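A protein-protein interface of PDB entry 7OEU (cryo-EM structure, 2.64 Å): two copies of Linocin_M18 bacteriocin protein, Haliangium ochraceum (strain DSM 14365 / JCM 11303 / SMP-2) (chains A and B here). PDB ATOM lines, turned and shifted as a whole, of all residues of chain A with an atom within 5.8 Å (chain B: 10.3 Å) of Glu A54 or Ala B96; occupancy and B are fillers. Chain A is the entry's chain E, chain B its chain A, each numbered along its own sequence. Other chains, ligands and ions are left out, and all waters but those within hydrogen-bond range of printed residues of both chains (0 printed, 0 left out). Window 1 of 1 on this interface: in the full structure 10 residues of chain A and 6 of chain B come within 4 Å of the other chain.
The backbone carbonyl oxygen (O) of Arg B94 is in hydrogen-bond range of the side-chain amide nitrogen (ND2) of Asn A51. NH2 of Arg A70 sits at hydrogen-bond distance from O of Arg B94, 3.0 Å away.
The backbone NH of Ala B96 sits at hydrogen-bond distance from the backbone carbonyl oxygen of Ser B91. The side-chain amide oxygen (OD1) of Asn A51 is in hydrogen-bond range of the backbone NH (N) of Gly A53. The side-chain amide oxygen of Asn A51 lies within hydrogen-bond range of the guanidinium group of Arg A70 (2.8 Å). The backbone NH of Glu A54 sits close to the side-chain hydroxyl of Thr A52 (3.3 Å). OG1 of Thr A52 lies within hydrogen-bond range of O of Gln A71, at 2.9 Å. O of Glu A54 lies within hydrogen-bond range of N of Gln A71, 3.0 Å away.
Among the printed residues, merely in contact across the chains: Thr A52 with Ala B96 (3.4 Å), Gly A53 with Ser B91 (3.8 Å), Gly A53 with Arg B94 (3.4 Å), Gly A53 with Ala B96 (3.8 Å), Glu A54 with Ser B91 (3.96 Å), Glu A54 with Ala B96 (3.1 Å) and Leu A55 with Arg B94 (3.4 Å).
Glu A54 touches just these residues of chain B: Ser B91 and Ala B96. Ala B96 touches just these residues of chain A: Thr A52 (3.4 Å), Gly A53 (3.8 Å) and Glu A54 (3.1 Å). Of the printed residues of chain B, Thr A52 touches Ala B96. Of chain B, only Ser B91 (3.8 Å), Arg B94 (3.4 Å) and Ala B96 (3.8 Å) come within 4 Å of Gly A53. Gln A71 touches none of the printed residues of chain B. Of the printed residues of chain A, Arg B94 touches Asn A51 (3.2 Å), Gly A53 (3.4 Å), Leu A55 (3.4 Å) and Arg A70 (3.0 Å). Printed residues of chain A within 4 Å of Ser B91: Gly A53 and Glu A54. Printed residues of chain B within 4 Å of Arg A70: Arg B94. Of the printed residues of chain B, Asn A51 touches Arg B94. Asn B98 touches none of the printed residues of chain A. Asp B100 touches none of the printed residues of chain A. The nearest residue of chain A that does not touch Ala B96 is Asn A51 (5.6 Å). The nearest printed residue of chain B that does not touch Arg A70 is Gly B95 (5.2 Å).
Hydrophobic or aromatic side chains of chain A that line the printed part of chain B: Leu A55. Hydrophobic or aromatic side chains of chain B within 4 Å of the printed part of chain A: Ala B96.
No position is printed for both chains.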
ATOM      1  N   ASN A  51      27.619  24.581  -0.781  1.00  0.00           N
ATOM      2  CA  ASN A  51      27.474  23.225  -0.268  1.00  0.00           C
ATOM      3  C   ASN A  51      26.007  22.819  -0.300  1.00  0.00           C
ATOM      4  O   ASN A  51      25.163  23.469   0.321  1.00  0.00           O
ATOM      5  CB  ASN A  51      28.030  23.140   1.151  1.00  0.00           C
ATOM      6  CG  ASN A  51      27.574  21.895   1.887  1.00  0.00           C
ATOM      7  OD1 ASN A  51      27.600  20.793   1.346  1.00  0.00           O
ATOM      8  ND2 ASN A  51      27.149  22.069   3.130  1.00  0.00           N
ATOM      9  N   THR A  52      25.702  21.749  -1.027  1.00  0.00           N
ATOM     10  CA  THR A  52      24.332  21.265  -1.122  1.00  0.00           C
ATOM     11  C   THR A  52      23.962  20.299  -0.006  1.00  0.00           C
ATOM     12  O   THR A  52      22.771  20.087   0.240  1.00  0.00           O
ATOM     13  CB  THR A  52      24.098  20.582  -2.472  1.00  0.00           C
ATOM     14  OG1 THR A  52      24.775  19.320  -2.497  1.00  0.00           O
ATOM     15  CG2 THR A  52      24.615  21.450  -3.604  1.00  0.00           C
ATOM     16  N   GLY A  53      24.944  19.723   0.680  1.00  0.00           N
ATOM     17  CA  GLY A  53      24.683  18.748   1.712  1.00  0.00           C
ATOM     18  C   GLY A  53      24.389  17.353   1.216  1.00  0.00           C
ATOM     19  O   GLY A  53      24.094  16.476   2.034  1.00  0.00           O
ATOM     20  N   GLU A  54      24.453  17.116  -0.088  1.00  0.00           N
ATOM     21  CA  GLU A  54      24.202  15.802  -0.653  1.00  0.00           C
ATOM     22  C   GLU A  54      25.502  15.038  -0.855  1.00  0.00           C
ATOM     23  O   GLU A  54      26.583  15.616  -0.985  1.00  0.00           O
ATOM     24  CB  GLU A  54      23.459  15.901  -1.989  1.00  0.00           C
ATOM     25  CG  GLU A  54      22.244  16.807  -1.998  1.00  0.00           C
ATOM     26  CD  GLU A  54      21.448  16.755  -0.713  1.00  0.00           C
ATOM     27  OE1 GLU A  54      21.088  15.644  -0.266  1.00  0.00           O
ATOM     28  OE2 GLU A  54      21.179  17.833  -0.149  1.00  0.00           O
ATOM     29  N   LEU A  55      25.375  13.719  -0.883  1.00  0.00           N
ATOM     30  CA  LEU A  55      26.469  12.817  -1.187  1.00  0.00           C
ATOM     31  C   LEU A  55      26.111  12.000  -2.417  1.00  0.00           C
ATOM     32  O   LEU A  55      24.944  11.675  -2.644  1.00  0.00           O
ATOM     33  CB  LEU A  55      26.760  11.880  -0.012  1.00  0.00           C
ATOM     34  CG  LEU A  55      27.566  12.447   1.152  1.00  0.00           C
ATOM     35  CD1 LEU A  55      27.396  11.566   2.367  1.00  0.00           C
ATOM     36  CD2 LEU A  55      29.032  12.563   0.776  1.00  0.00           C
ATOM     37  N   ARG A  56      27.118  11.676  -3.216  1.00  0.00           N
ATOM     38  CA  ARG A  56      26.924  10.815  -4.361  1.00  0.00           C
ATOM     39  C   ARG A  56      27.775   9.566  -4.200  1.00  0.00           C
ATOM     40  O   ARG A  56      28.969   9.668  -3.884  1.00  0.00           O
ATOM     41  CB  ARG A  56      27.284  11.523  -5.671  1.00  0.00           C
ATOM     42  CG  ARG A  56      26.417  11.102  -6.841  1.00  0.00           C
ATOM     43  CD  ARG A  56      26.978  11.564  -8.179  1.00  0.00           C
ATOM     44  NE  ARG A  56      28.407  11.293  -8.317  1.00  0.00           N
ATOM     45  CZ  ARG A  56      29.351  12.228  -8.314  1.00  0.00           C
ATOM     46  NH1 ARG A  56      29.023  13.504  -8.182  1.00  0.00           N
ATOM     47  NH2 ARG A  56      30.626  11.887  -8.447  1.00  0.00           N
ATOM     48  N   LEU A  69      31.203  10.947  -2.485  1.00  0.00           N
ATOM     49  CA  LEU A  69      31.729  12.265  -2.799  1.00  0.00           C
ATOM     50  C   LEU A  69      30.702  13.329  -2.454  1.00  0.00           C
ATOM     51  O   LEU A  69      29.516  13.182  -2.755  1.00  0.00           O
ATOM     52  CB  LEU A  69      32.108  12.367  -4.275  1.00  0.00           C
ATOM     53  CG  LEU A  69      33.596  12.242  -4.596  1.00  0.00           C
ATOM     54  CD1 LEU A  69      33.841  12.566  -6.052  1.00  0.00           C
ATOM     55  CD2 LEU A  69      34.413  13.151  -3.702  1.00  0.00           C
ATOM     56  N   ARG A  70      31.155  14.398  -1.817  1.00  0.00           N
ATOM     57  CA  ARG A  70      30.258  15.490  -1.479  1.00  0.00           C
ATOM     58  C   ARG A  70      29.940  16.306  -2.723  1.00  0.00           C
ATOM     59  O   ARG A  70      30.802  16.533  -3.574  1.00  0.00           O
ATOM     60  CB  ARG A  70      30.873  16.366  -0.392  1.00  0.00           C
ATOM     61  CG  ARG A  70      31.035  15.599   0.897  1.00  0.00           C
ATOM     62  CD  ARG A  70      30.819  16.419   2.139  1.00  0.00           C
ATOM     63  NE  ARG A  70      29.605  17.221   2.111  1.00  0.00           N
ATOM     64  CZ  ARG A  70      29.158  17.895   3.162  1.00  0.00           C
ATOM     65  NH1 ARG A  70      29.816  17.838   4.307  1.00  0.00           N
ATOM     66  NH2 ARG A  70      28.052  18.612   3.076  1.00  0.00           N
ATOM     67  N   GLN A  71      28.686  16.724  -2.835  1.00  0.00           N
ATOM     68  CA  GLN A  71      28.200  17.454  -3.995  1.00  0.00           C
ATOM     69  C   GLN A  71      28.153  18.938  -3.684  1.00  0.00           C
ATOM     70  O   GLN A  71      27.698  19.348  -2.613  1.00  0.00           O
ATOM     71  CB  GLN A  71      26.819  16.956  -4.415  1.00  0.00           C
ATOM     72  CG  GLN A  71      26.788  15.472  -4.674  1.00  0.00           C
ATOM     73  CD  GLN A  71      27.821  15.059  -5.698  1.00  0.00           C
ATOM     74  OE1 GLN A  71      27.776  15.492  -6.846  1.00  0.00           O
ATOM     75  NE2 GLN A  71      28.783  14.250  -5.276  1.00  0.00           N
ATOM     76  N   ARG A 253      20.255  28.130  -7.604  1.00  0.00           N
ATOM     77  CA  ARG A 253      19.758  26.787  -7.356  1.00  0.00           C
ATOM     78  C   ARG A 253      18.237  26.783  -7.339  1.00  0.00           C
ATOM     79  O   ARG A 253      17.606  27.674  -6.762  1.00  0.00           O
ATOM     80  CB  ARG A 253      20.291  26.241  -6.029  1.00  0.00           C
ATOM     81  CG  ARG A 253      21.741  25.809  -6.074  1.00  0.00           C
ATOM     82  CD  ARG A 253      22.272  25.531  -4.685  1.00  0.00           C
ATOM     83  NE  ARG A 253      21.871  24.209  -4.221  1.00  0.00           N
ATOM     84  CZ  ARG A 253      21.436  23.949  -2.994  1.00  0.00           C
ATOM     85  NH1 ARG A 253      21.352  24.920  -2.099  1.00  0.00           N
ATOM     86  NH2 ARG A 253      21.090  22.715  -2.664  1.00  0.00           N
ATOM     87  N   VAL B  12      18.551  13.198  13.921  1.00  0.00           N
ATOM     88  CA  VAL B  12      19.253  14.332  14.520  1.00  0.00           C
ATOM     89  C   VAL B  12      18.240  15.433  14.817  1.00  0.00           C
ATOM     90  O   VAL B  12      17.176  15.478  14.187  1.00  0.00           O
ATOM     91  CB  VAL B  12      20.396  14.833  13.618  1.00  0.00           C
ATOM     92  CG1 VAL B  12      21.363  13.701  13.305  1.00  0.00           C
ATOM     93  CG2 VAL B  12      19.855  15.459  12.341  1.00  0.00           C
ATOM     94  N   ASP B  14      17.913  18.602  14.107  1.00  0.00           N
ATOM     95  CA  ASP B  14      17.487  19.459  13.006  1.00  0.00           C
ATOM     96  C   ASP B  14      16.561  18.726  12.046  1.00  0.00           C
ATOM     97  O   ASP B  14      15.649  19.337  11.480  1.00  0.00           O
ATOM     98  CB  ASP B  14      18.703  20.017  12.268  1.00  0.00           C
ATOM     99  CG  ASP B  14      19.477  21.012  13.099  1.00  0.00           C
ATOM    100  OD1 ASP B  14      18.859  21.684  13.952  1.00  0.00           O
ATOM    101  OD2 ASP B  14      20.704  21.131  12.902  1.00  0.00           O
ATOM    102  N   ALA B  15      16.771  17.425  11.854  1.00  0.00           N
ATOM    103  CA  ALA B  15      15.828  16.645  11.062  1.00  0.00           C
ATOM    104  C   ALA B  15      14.465  16.574  11.743  1.00  0.00           C
ATOM    105  O   ALA B  15      13.428  16.629  11.073  1.00  0.00           O
ATOM    106  CB  ALA B  15      16.393  15.251  10.800  1.00  0.00           C
ATOM    107  N   SER B  17      13.281  18.967  13.601  1.00  0.00           N
ATOM    108  CA  SER B  17      12.719  20.289  13.349  1.00  0.00           C
ATOM    109  C   SER B  17      12.122  20.379  11.950  1.00  0.00           C
ATOM    110  O   SER B  17      11.037  20.939  11.769  1.00  0.00           O
ATOM    111  CB  SER B  17      13.788  21.361  13.542  1.00  0.00           C
ATOM    112  OG  SER B  17      14.114  21.507  14.910  1.00  0.00           O
ATOM    113  N   ALA B  18      12.817  19.834  10.952  1.00  0.00           N
ATOM    114  CA  ALA B  18      12.300  19.867   9.586  1.00  0.00           C
ATOM    115  C   ALA B  18      11.004  19.072   9.460  1.00  0.00           C
ATOM    116  O   ALA B  18      10.046  19.526   8.820  1.00  0.00           O
ATOM    117  CB  ALA B  18      13.352  19.339   8.613  1.00  0.00           C
ATOM    118  N   ILE B  19      10.957  17.882  10.065  1.00  0.00           N
ATOM    119  CA  ILE B  19       9.744  17.067  10.027  1.00  0.00           C
ATOM    120  C   ILE B  19       8.585  17.813  10.677  1.00  0.00           C
ATOM    121  O   ILE B  19       7.468  17.870  10.138  1.00  0.00           O
ATOM    122  CB  ILE B  19       9.995  15.711  10.712  1.00  0.00           C
ATOM    123  CG1 ILE B  19      10.954  14.857   9.887  1.00  0.00           C
ATOM    124  CG2 ILE B  19       8.688  14.971  10.949  1.00  0.00           C
ATOM    125  CD1 ILE B  19      11.691  13.826  10.701  1.00  0.00           C
ATOM    126  N   ASP B  85      13.281   8.003   4.934  1.00  0.00           N
ATOM    127  CA  ASP B  85      14.598   7.443   4.674  1.00  0.00           C
ATOM    128  C   ASP B  85      15.611   8.021   5.652  1.00  0.00           C
ATOM    129  O   ASP B  85      15.676   9.237   5.846  1.00  0.00           O
ATOM    130  CB  ASP B  85      15.019   7.736   3.236  1.00  0.00           C
ATOM    131  CG  ASP B  85      16.023   6.739   2.710  1.00  0.00           C
ATOM    132  OD1 ASP B  85      15.770   5.524   2.823  1.00  0.00           O
ATOM    133  OD2 ASP B  85      17.066   7.172   2.181  1.00  0.00           O
ATOM    134  N   VAL B  86      16.403   7.144   6.269  1.00  0.00           N
ATOM    135  CA  VAL B  86      17.354   7.593   7.281  1.00  0.00           C
ATOM    136  C   VAL B  86      18.450   8.448   6.656  1.00  0.00           C
ATOM    137  O   VAL B  86      18.900   9.427   7.256  1.00  0.00           O
ATOM    138  CB  VAL B  86      17.932   6.390   8.049  1.00  0.00           C
ATOM    139  CG1 VAL B  86      18.894   6.861   9.123  1.00  0.00           C
ATOM    140  CG2 VAL B  86      16.814   5.578   8.673  1.00  0.00           C
ATOM    141  N   THR B  87      18.895   8.103   5.445  1.00  0.00           N
ATOM    142  CA  THR B  87      19.949   8.885   4.799  1.00  0.00           C
ATOM    143  C   THR B  87      19.468  10.289   4.446  1.00  0.00           C
ATOM    144  O   THR B  87      20.228  11.260   4.560  1.00  0.00           O
ATOM    145  CB  THR B  87      20.461   8.169   3.551  1.00  0.00           C
ATOM    146  OG1 THR B  87      19.364   7.871   2.678  1.00  0.00           O
ATOM    147  CG2 THR B  87      21.166   6.880   3.929  1.00  0.00           C
ATOM    148  N   GLU B  88      18.213  10.417   4.012  1.00  0.00           N
ATOM    149  CA  GLU B  88      17.666  11.737   3.728  1.00  0.00           C
ATOM    150  C   GLU B  88      17.638  12.599   4.983  1.00  0.00           C
ATOM    151  O   GLU B  88      17.909  13.803   4.923  1.00  0.00           O
ATOM    152  CB  GLU B  88      16.266  11.610   3.131  1.00  0.00           C
ATOM    153  CG  GLU B  88      16.249  11.130   1.692  1.00  0.00           C
ATOM    154  CD  GLU B  88      16.489  12.250   0.695  1.00  0.00           C
ATOM    155  OE1 GLU B  88      16.617  11.955  -0.510  1.00  0.00           O
ATOM    156  OE2 GLU B  88      16.546  13.424   1.114  1.00  0.00           O
ATOM    157  N   LEU B  89      17.310  12.002   6.127  1.00  0.00           N
ATOM    158  CA  LEU B  89      17.324  12.751   7.377  1.00  0.00           C
ATOM    159  C   LEU B  89      18.745  13.052   7.833  1.00  0.00           C
ATOM    160  O   LEU B  89      18.989  14.092   8.453  1.00  0.00           O
ATOM    161  CB  LEU B  89      16.560  11.982   8.453  1.00  0.00           C
ATOM    162  CG  LEU B  89      15.068  11.761   8.189  1.00  0.00           C
ATOM    163  CD1 LEU B  89      14.437  10.950   9.300  1.00  0.00           C
ATOM    164  CD2 LEU B  89      14.343  13.087   8.010  1.00  0.00           C
ATOM    165  N   ASP B  90      19.690  12.159   7.538  1.00  0.00           N
ATOM    166  CA  ASP B  90      21.088  12.407   7.868  1.00  0.00           C
ATOM    167  C   ASP B  90      21.640  13.581   7.074  1.00  0.00           C
ATOM    168  O   ASP B  90      22.466  14.347   7.582  1.00  0.00           O
ATOM    169  CB  ASP B  90      21.922  11.154   7.609  1.00  0.00           C
ATOM    170  CG  ASP B  90      21.620  10.038   8.587  1.00  0.00           C
ATOM    171  OD1 ASP B  90      21.331  10.336   9.763  1.00  0.00           O
ATOM    172  OD2 ASP B  90      21.671   8.860   8.179  1.00  0.00           O
ATOM    173  N   SER B  91      21.198  13.731   5.823  1.00  0.00           N
ATOM    174  CA  SER B  91      21.692  14.815   4.978  1.00  0.00           C
ATOM    175  C   SER B  91      21.425  16.187   5.580  1.00  0.00           C
ATOM    176  O   SER B  91      22.140  17.140   5.257  1.00  0.00           O
ATOM    177  CB  SER B  91      21.066  14.725   3.586  1.00  0.00           C
ATOM    178  OG  SER B  91      19.732  15.190   3.594  1.00  0.00           O
ATOM    179  N   VAL B  92      20.423  16.306   6.451  1.00  0.00           N
ATOM    180  CA  VAL B  92      20.173  17.568   7.142  1.00  0.00           C
ATOM    181  C   VAL B  92      21.389  17.973   7.963  1.00  0.00           C
ATOM    182  O   VAL B  92      21.745  19.156   8.034  1.00  0.00           O
ATOM    183  CB  VAL B  92      18.908  17.449   8.016  1.00  0.00           C
ATOM    184  CG1 VAL B  92      18.823  18.594   9.002  1.00  0.00           C
ATOM    185  CG2 VAL B  92      17.667  17.403   7.146  1.00  0.00           C
ATOM    186  N   ALA B  93      22.052  17.001   8.590  1.00  0.00           N
ATOM    187  CA  ALA B  93      23.243  17.287   9.379  1.00  0.00           C
ATOM    188  C   ALA B  93      24.412  17.767   8.528  1.00  0.00           C
ATOM    189  O   ALA B  93      25.309  18.431   9.054  1.00  0.00           O
ATOM    190  CB  ALA B  93      23.656  16.049  10.175  1.00  0.00           C
ATOM    191  N   ARG B  94      24.427  17.454   7.236  1.00  0.00           N
ATOM    192  CA  ARG B  94      25.473  17.927   6.341  1.00  0.00           C
ATOM    193  C   ARG B  94      25.127  19.250   5.672  1.00  0.00           C
ATOM    194  O   ARG B  94      25.874  19.702   4.802  1.00  0.00           O
ATOM    195  CB  ARG B  94      25.778  16.872   5.279  1.00  0.00           C
ATOM    196  CG  ARG B  94      26.533  15.682   5.808  1.00  0.00           C
ATOM    197  CD  ARG B  94      26.841  14.697   4.710  1.00  0.00           C
ATOM    198  NE  ARG B  94      27.130  13.372   5.241  1.00  0.00           N
ATOM    199  CZ  ARG B  94      26.210  12.448   5.489  1.00  0.00           C
ATOM    200  NH1 ARG B  94      24.932  12.701   5.258  1.00  0.00           N
ATOM    201  NH2 ARG B  94      26.570  11.268   5.969  1.00  0.00           N
ATOM    202  N   GLY B  95      24.021  19.873   6.053  1.00  0.00           N
ATOM    203  CA  GLY B  95      23.642  21.157   5.510  1.00  0.00           C
ATOM    204  C   GLY B  95      22.591  21.131   4.424  1.00  0.00           C
ATOM    205  O   GLY B  95      22.298  22.186   3.854  1.00  0.00           O
ATOM    206  N   ALA B  96      22.023  19.972   4.116  1.00  0.00           N
ATOM    207  CA  ALA B  96      20.952  19.908   3.133  1.00  0.00           C
ATOM    208  C   ALA B  96      19.715  20.628   3.651  1.00  0.00           C
ATOM    209  O   ALA B  96      19.343  20.496   4.819  1.00  0.00           O
ATOM    210  CB  ALA B  96      20.621  18.457   2.799  1.00  0.00           C
ATOM    211  N   THR B  97      19.078  21.403   2.774  1.00  0.00           N
ATOM    212  CA  THR B  97      17.922  22.204   3.147  1.00  0.00           C
ATOM    213  C   THR B  97      16.600  21.644   2.644  1.00  0.00           C
ATOM    214  O   THR B  97      15.547  22.109   3.088  1.00  0.00           O
ATOM    215  CB  THR B  97      18.075  23.641   2.630  1.00  0.00           C
ATOM    216  OG1 THR B  97      18.113  23.635   1.199  1.00  0.00           O
ATOM    217  CG2 THR B  97      19.347  24.267   3.164  1.00  0.00           C
ATOM    218  N   ASN B  98      16.618  20.671   1.739  1.00  0.00           N
ATOM    219  CA  ASN B  98      15.399  20.103   1.167  1.00  0.00           C
ATOM    220  C   ASN B  98      15.454  18.583   1.195  1.00  0.00           C
ATOM    221  O   ASN B  98      15.536  17.932   0.146  1.00  0.00           O
ATOM    222  CB  ASN B  98      15.188  20.613  -0.258  1.00  0.00           C
ATOM    223  CG  ASN B  98      14.969  22.103  -0.310  1.00  0.00           C
ATOM    224  OD1 ASN B  98      15.785  22.840  -0.856  1.00  0.00           O
ATOM    225  ND2 ASN B  98      13.857  22.560   0.251  1.00  0.00           N
ATOM    226  N   PRO B  99      15.406  17.979   2.379  1.00  0.00           N
ATOM    227  CA  PRO B  99      15.276  16.523   2.446  1.00  0.00           C
ATOM    228  C   PRO B  99      13.902  16.078   1.972  1.00  0.00           C
ATOM    229  O   PRO B  99      12.924  16.826   2.028  1.00  0.00           O
ATOM    230  CB  PRO B  99      15.478  16.221   3.933  1.00  0.00           C
ATOM    231  CG  PRO B  99      14.999  17.451   4.609  1.00  0.00           C
ATOM    232  CD  PRO B  99      15.417  18.585   3.722  1.00  0.00           C
ATOM    233  N   ASP B 100      13.839  14.838   1.498  1.00  0.00           N
ATOM    234  CA  ASP B 100      12.596  14.259   0.996  1.00  0.00           C
ATOM    235  C   ASP B 100      11.676  13.944   2.169  1.00  0.00           C
ATOM    236  O   ASP B 100      11.872  12.960   2.884  1.00  0.00           O
ATOM    237  CB  ASP B 100      12.891  13.010   0.175  1.00  0.00           C
ATOM    238  CG  ASP B 100      11.633  12.307  -0.289  1.00  0.00           C
ATOM    239  OD1 ASP B 100      10.603  12.984  -0.472  1.00  0.00           O
ATOM    240  OD2 ASP B 100      11.677  11.075  -0.475  1.00  0.00           O
ATOM    241  N   LEU B 101      10.661  14.779   2.367  1.00  0.00           N
ATOM    242  CA  LEU B 101       9.683  14.621   3.435  1.00  0.00           C
ATOM    243  C   LEU B 101       8.277  14.468   2.866  1.00  0.00           C
ATOM    244  O   LEU B 101       7.305  14.986   3.412  1.00  0.00           O
ATOM    245  CB  LEU B 101       9.748  15.800   4.403  1.00  0.00           C
ATOM    246  CG  LEU B 101      11.108  16.049   5.057  1.00  0.00           C
ATOM    247  CD1 LEU B 101      11.073  17.292   5.923  1.00  0.00           C
ATOM    248  CD2 LEU B 101      11.544  14.839   5.866  1.00  0.00           C
